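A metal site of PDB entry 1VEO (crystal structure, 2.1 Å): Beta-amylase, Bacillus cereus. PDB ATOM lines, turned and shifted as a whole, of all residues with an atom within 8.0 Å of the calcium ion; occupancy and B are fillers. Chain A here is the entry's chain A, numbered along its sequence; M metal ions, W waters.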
ATOM      1  N   TRP A  52     -18.719  27.813 -12.883  1.00  0.00           N
ATOM      2  CA  TRP A  52     -19.635  28.227 -13.922  1.00  0.00           C
ATOM      3  C   TRP A  52     -20.806  28.935 -13.234  1.00  0.00           C
ATOM      4  O   TRP A  52     -21.298  29.958 -13.706  1.00  0.00           O
ATOM      5  CB  TRP A  52     -20.116  27.004 -14.714  1.00  0.00           C
ATOM      6  CG  TRP A  52     -20.892  27.344 -15.947  1.00  0.00           C
ATOM      7  CD1 TRP A  52     -21.018  28.571 -16.544  1.00  0.00           C
ATOM      8  CD2 TRP A  52     -21.661  26.432 -16.754  1.00  0.00           C
ATOM      9  NE1 TRP A  52     -21.815  28.491 -17.650  1.00  0.00           N
ATOM     10  CE2 TRP A  52     -22.236  27.192 -17.808  1.00  0.00           C
ATOM     11  CE3 TRP A  52     -21.931  25.065 -16.672  1.00  0.00           C
ATOM     12  CZ2 TRP A  52     -23.049  26.622 -18.791  1.00  0.00           C
ATOM     13  CZ3 TRP A  52     -22.754  24.485 -17.652  1.00  0.00           C
ATOM     14  CH2 TRP A  52     -23.307  25.271 -18.690  1.00  0.00           C
ATOM     15  N   GLU A  56     -21.687  32.788 -14.939  1.00  0.00           N
ATOM     16  CA  GLU A  56     -22.834  32.949 -15.832  1.00  0.00           C
ATOM     17  C   GLU A  56     -24.111  32.643 -15.049  1.00  0.00           C
ATOM     18  O   GLU A  56     -25.001  31.973 -15.560  1.00  0.00           O
ATOM     19  CB  GLU A  56     -22.711  31.996 -17.027  1.00  0.00           C
ATOM     20  CG  GLU A  56     -23.269  32.532 -18.340  1.00  0.00           C
ATOM     21  CD  GLU A  56     -23.210  31.509 -19.478  1.00  0.00           C
ATOM     22  OE1 GLU A  56     -22.215  30.759 -19.572  1.00  0.00           O
ATOM     23  OE2 GLU A  56     -24.161  31.462 -20.286  1.00  0.00           O
ATOM     24  N   GLY A  59     -28.049  34.569 -16.366  1.00  0.00           N
ATOM     25  CA  GLY A  59     -28.690  33.957 -17.508  1.00  0.00           C
ATOM     26  C   GLY A  59     -27.699  33.721 -18.631  1.00  0.00           C
ATOM     27  O   GLY A  59     -26.524  34.092 -18.528  1.00  0.00           O
ATOM     28  N   ASP A  60     -28.165  33.110 -19.706  1.00  0.00           N
ATOM     29  CA  ASP A  60     -27.312  32.822 -20.846  1.00  0.00           C
ATOM     30  C   ASP A  60     -26.626  34.089 -21.345  1.00  0.00           C
ATOM     31  O   ASP A  60     -27.266  35.127 -21.550  1.00  0.00           O
ATOM     32  CB  ASP A  60     -28.145  32.170 -21.961  1.00  0.00           C
ATOM     33  CG  ASP A  60     -27.285  31.723 -23.134  1.00  0.00           C
ATOM     34  OD1 ASP A  60     -26.127  31.331 -22.925  1.00  0.00           O
ATOM     35  OD2 ASP A  60     -27.792  31.755 -24.284  1.00  0.00           O
ATOM     36  N   GLN A  61     -25.310  33.997 -21.498  1.00  0.00           N
ATOM     37  CA  GLN A  61     -24.485  35.103 -21.977  1.00  0.00           C
ATOM     38  C   GLN A  61     -24.335  36.284 -21.013  1.00  0.00           C
ATOM     39  O   GLN A  61     -23.775  37.317 -21.385  1.00  0.00           O
ATOM     40  CB  GLN A  61     -25.004  35.597 -23.319  1.00  0.00           C
ATOM     41  CG  GLN A  61     -24.886  34.564 -24.433  1.00  0.00           C
ATOM     42  CD  GLN A  61     -23.503  33.938 -24.518  1.00  0.00           C
ATOM     43  OE1 GLN A  61     -23.151  33.038 -23.750  1.00  0.00           O
ATOM     44  NE2 GLN A  61     -22.695  34.423 -25.462  1.00  0.00           N
ATOM     45  N   GLN A  62     -24.844  36.133 -19.787  1.00  0.00           N
ATOM     46  CA  GLN A  62     -24.722  37.181 -18.777  1.00  0.00           C
ATOM     47  C   GLN A  62     -23.531  36.812 -17.889  1.00  0.00           C
ATOM     48  O   GLN A  62     -23.693  36.222 -16.818  1.00  0.00           O
ATOM     49  CB  GLN A  62     -25.986  37.273 -17.948  1.00  0.00           C
ATOM     50  CG  GLN A  62     -27.080  38.070 -18.621  1.00  0.00           C
ATOM     51  CD  GLN A  62     -28.323  38.148 -17.772  1.00  0.00           C
ATOM     52  OE1 GLN A  62     -29.119  37.213 -17.715  1.00  0.00           O
ATOM     53  NE2 GLN A  62     -28.488  39.281 -17.086  1.00  0.00           N
ATOM     54  N   PHE A  63     -22.338  37.170 -18.351  1.00  0.00           N
ATOM     55  CA  PHE A  63     -21.099  36.831 -17.669  1.00  0.00           C
ATOM     56  C   PHE A  63     -20.628  37.785 -16.577  1.00  0.00           C
ATOM     57  O   PHE A  63     -20.967  38.962 -16.561  1.00  0.00           O
ATOM     58  CB  PHE A  63     -19.988  36.661 -18.706  1.00  0.00           C
ATOM     59  CG  PHE A  63     -20.233  35.554 -19.684  1.00  0.00           C
ATOM     60  CD1 PHE A  63     -20.227  34.223 -19.272  1.00  0.00           C
ATOM     61  CD2 PHE A  63     -20.476  35.832 -21.021  1.00  0.00           C
ATOM     62  CE1 PHE A  63     -20.461  33.186 -20.174  1.00  0.00           C
ATOM     63  CE2 PHE A  63     -20.705  34.806 -21.935  1.00  0.00           C
ATOM     64  CZ  PHE A  63     -20.698  33.472 -21.502  1.00  0.00           C
ATOM     65  N   TRP A 106     -30.495  28.140 -15.069  1.00  0.00           N
ATOM     66  CA  TRP A 106     -31.191  28.303 -16.345  1.00  0.00           C
ATOM     67  C   TRP A 106     -30.816  27.283 -17.411  1.00  0.00           C
ATOM     68  O   TRP A 106     -31.608  27.027 -18.322  1.00  0.00           O
ATOM     69  CB  TRP A 106     -30.959  29.713 -16.893  1.00  0.00           C
ATOM     70  CG  TRP A 106     -29.526  30.074 -17.046  1.00  0.00           C
ATOM     71  CD1 TRP A 106     -28.772  30.796 -16.164  1.00  0.00           C
ATOM     72  CD2 TRP A 106     -28.660  29.727 -18.135  1.00  0.00           C
ATOM     73  NE1 TRP A 106     -27.485  30.920 -16.641  1.00  0.00           N
ATOM     74  CE2 TRP A 106     -27.384  30.276 -17.845  1.00  0.00           C
ATOM     75  CE3 TRP A 106     -28.837  29.003 -19.319  1.00  0.00           C
ATOM     76  CZ2 TRP A 106     -26.295  30.116 -18.696  1.00  0.00           C
ATOM     77  CZ3 TRP A 106     -27.739  28.852 -20.173  1.00  0.00           C
ATOM     78  CH2 TRP A 106     -26.493  29.401 -19.855  1.00  0.00           C
ATOM     79  N   VAL A 107     -29.625  26.718 -17.310  1.00  0.00           N
ATOM     80  CA  VAL A 107     -29.192  25.755 -18.316  1.00  0.00           C
ATOM     81  C   VAL A 107     -30.165  24.581 -18.452  1.00  0.00           C
ATOM     82  O   VAL A 107     -30.374  24.063 -19.545  1.00  0.00           O
ATOM     83  CB  VAL A 107     -27.772  25.215 -17.989  1.00  0.00           C
ATOM     84  CG1 VAL A 107     -27.803  24.334 -16.757  1.00  0.00           C
ATOM     85  CG2 VAL A 107     -27.234  24.444 -19.177  1.00  0.00           C
ATOM     86  N   GLN A 110     -33.119  24.703 -21.165  1.00  0.00           N
ATOM     87  CA  GLN A 110     -32.885  24.670 -22.601  1.00  0.00           C
ATOM     88  C   GLN A 110     -33.311  23.350 -23.244  1.00  0.00           C
ATOM     89  O   GLN A 110     -33.099  23.148 -24.436  1.00  0.00           O
ATOM     90  CB  GLN A 110     -31.410  24.942 -22.898  1.00  0.00           C
ATOM     91  CG  GLN A 110     -31.025  26.397 -22.736  1.00  0.00           C
ATOM     92  CD  GLN A 110     -29.709  26.725 -23.409  1.00  0.00           C
ATOM     93  OE1 GLN A 110     -29.334  27.892 -23.528  1.00  0.00           O
ATOM     94  NE2 GLN A 110     -28.988  25.696 -23.846  1.00  0.00           N
ATOM     95  N   VAL A 137     -25.804  21.027 -26.588  1.00  0.00           N
ATOM     96  CA  VAL A 137     -25.870  22.075 -25.568  1.00  0.00           C
ATOM     97  C   VAL A 137     -24.468  22.374 -25.025  1.00  0.00           C
ATOM     98  O   VAL A 137     -24.135  23.526 -24.743  1.00  0.00           O
ATOM     99  CB  VAL A 137     -26.780  21.636 -24.398  1.00  0.00           C
ATOM    100  CG1 VAL A 137     -26.595  22.571 -23.201  1.00  0.00           C
ATOM    101  CG2 VAL A 137     -28.234  21.638 -24.856  1.00  0.00           C
ATOM    102  N   LYS A 140     -22.482  24.544 -27.462  1.00  0.00           N
ATOM    103  CA  LYS A 140     -22.939  25.906 -27.347  1.00  0.00           C
ATOM    104  C   LYS A 140     -22.430  26.579 -26.076  1.00  0.00           C
ATOM    105  O   LYS A 140     -21.612  27.501 -26.135  1.00  0.00           O
ATOM    106  CB  LYS A 140     -24.459  25.971 -27.353  1.00  0.00           C
ATOM    107  CG  LYS A 140     -24.991  27.379 -27.212  1.00  0.00           C
ATOM    108  CD  LYS A 140     -26.474  27.411 -26.898  1.00  0.00           C
ATOM    109  CE  LYS A 140     -26.976  28.844 -26.745  1.00  0.00           C
ATOM    110  NZ  LYS A 140     -26.350  29.559 -25.599  1.00  0.00           N
ATOM    111  N   GLU A 141     -22.899  26.108 -24.932  1.00  0.00           N
ATOM    112  CA  GLU A 141     -22.522  26.683 -23.642  1.00  0.00           C
ATOM    113  C   GLU A 141     -21.034  26.713 -23.312  1.00  0.00           C
ATOM    114  O   GLU A 141     -20.516  27.773 -22.953  1.00  0.00           O
ATOM    115  CB  GLU A 141     -23.283  25.996 -22.508  1.00  0.00           C
ATOM    116  CG  GLU A 141     -24.801  26.113 -22.598  1.00  0.00           C
ATOM    117  CD  GLU A 141     -25.268  27.522 -22.941  1.00  0.00           C
ATOM    118  OE1 GLU A 141     -24.754  28.493 -22.354  1.00  0.00           O
ATOM    119  OE2 GLU A 141     -26.169  27.658 -23.799  1.00  0.00           O
ATOM    120  N   TYR A 142     -20.338  25.587 -23.431  1.00  0.00           N
ATOM    121  CA  TYR A 142     -18.902  25.576 -23.127  1.00  0.00           C
ATOM    122  C   TYR A 142     -18.197  26.439 -24.152  1.00  0.00           C
ATOM    123  O   TYR A 142     -17.254  27.165 -23.820  1.00  0.00           O
ATOM    124  CB  TYR A 142     -18.330  24.159 -23.154  1.00  0.00           C
ATOM    125  CG  TYR A 142     -18.730  23.271 -21.988  1.00  0.00           C
ATOM    126  CD1 TYR A 142     -19.990  23.373 -21.402  1.00  0.00           C
ATOM    127  CD2 TYR A 142     -17.876  22.266 -21.524  1.00  0.00           C
ATOM    128  CE1 TYR A 142     -20.398  22.504 -20.378  1.00  0.00           C
ATOM    129  CE2 TYR A 142     -18.263  21.385 -20.502  1.00  0.00           C
ATOM    130  CZ  TYR A 142     -19.536  21.502 -19.940  1.00  0.00           C
ATOM    131  OH  TYR A 142     -19.960  20.602 -18.983  1.00  0.00           O
ATOM    132  N   GLY A 143     -18.654  26.357 -25.407  1.00  0.00           N
ATOM    133  CA  GLY A 143     -18.061  27.156 -26.463  1.00  0.00           C
ATOM    134  C   GLY A 143     -18.125  28.631 -26.102  1.00  0.00           C
ATOM    135  O   GLY A 143     -17.103  29.336 -26.163  1.00  0.00           O
ATOM    136  N   GLU A 144     -19.302  29.093 -25.711  1.00  0.00           N
ATOM    137  CA  GLU A 144     -19.477  30.489 -25.337  1.00  0.00           C
ATOM    138  C   GLU A 144     -18.699  30.845 -24.065  1.00  0.00           C
ATOM    139  O   GLU A 144     -17.993  31.849 -24.025  1.00  0.00           O
ATOM    140  CB  GLU A 144     -20.967  30.793 -25.165  1.00  0.00           C
ATOM    141  CG  GLU A 144     -21.738  30.623 -26.463  1.00  0.00           C
ATOM    142  CD  GLU A 144     -23.234  30.700 -26.261  1.00  0.00           C
ATOM    143  OE1 GLU A 144     -23.720  30.233 -25.210  1.00  0.00           O
ATOM    144  OE2 GLU A 144     -23.929  31.193 -27.174  1.00  0.00           O
ATOM    145  N   LEU A 145     -18.816  30.000 -23.033  1.00  0.00           N
ATOM    146  CA  LEU A 145     -18.100  30.254 -21.781  1.00  0.00           C
ATOM    147  C   LEU A 145     -16.588  30.389 -21.998  1.00  0.00           C
ATOM    148  O   LEU A 145     -15.990  31.369 -21.569  1.00  0.00           O
ATOM    149  CB  LEU A 145     -18.365  29.145 -20.765  1.00  0.00           C
ATOM    150  CG  LEU A 145     -17.686  29.350 -19.410  1.00  0.00           C
ATOM    151  CD1 LEU A 145     -18.125  30.691 -18.824  1.00  0.00           C
ATOM    152  CD2 LEU A 145     -18.048  28.211 -18.463  1.00  0.00           C
ATOM    153  N   ALA A 148     -15.659  33.555 -23.880  1.00  0.00           N
ATOM    154  CA  ALA A 148     -15.917  34.745 -23.075  1.00  0.00           C
ATOM    155  C   ALA A 148     -14.801  34.875 -22.040  1.00  0.00           C
ATOM    156  O   ALA A 148     -14.271  35.969 -21.807  1.00  0.00           O
ATOM    157  CB  ALA A 148     -17.270  34.620 -22.366  1.00  0.00           C
HETATM  158 CA    CA M   1     -23.986  30.745 -22.778  1.00  0.00          CA
HETATM  159  O   HOH W   1     -21.922  29.669 -21.875  1.00  0.00           O
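OD2 of Asp 60 lies within salt-bridge range of NZ of Lys 140 (2.9 Å).
OE2 of Glu 141 lies within salt-bridge range of NZ of Lys 140, at 2.6 Å.
The side-chain carboxylate of Glu 141 sits close to the side-chain amide oxygen of Gln 110 (3.2 Å).
NZ of Lys 140 is in salt-bridge range of OE2 of Glu 144, 3.3 Å away.
The backbone carbonyl oxygen of Glu 56 is in hydrogen-bond range of the indole nitrogen of Trp 106 (2.9 Å).
NE1 of Trp 52 lies within hydrogen-bond range of OE1 of Glu 56, at 3.0 Å.
Lys 140 touches the calcium ion.
The nearest printed residue that does not touch the calcium ion is Trp 106 (4.1 Å).
The calcium ion is bound by the side-chain carboxylate of Asp 60 (2.2 Å), the side-chain carboxylate of Glu 141 (2.4 Å), water W1 (2.5 Å), the side-chain carboxylate of Glu 144 (2.5 Å), the side-chain carboxylate of Glu 56 (2.6 Å) and the side-chain amide oxygen of Gln 61 (2.6 Å).
The calcium ion has six donor atoms within binding distance.
Water W1 lies within hydrogen-bond range of the side-chain carboxylate (OE1) of Glu 56 (2.6 Å), the backbone carbonyl oxygen (O) of Glu 141 (2.6 Å) and the backbone NH (N) of Leu 145 (3.3 Å).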
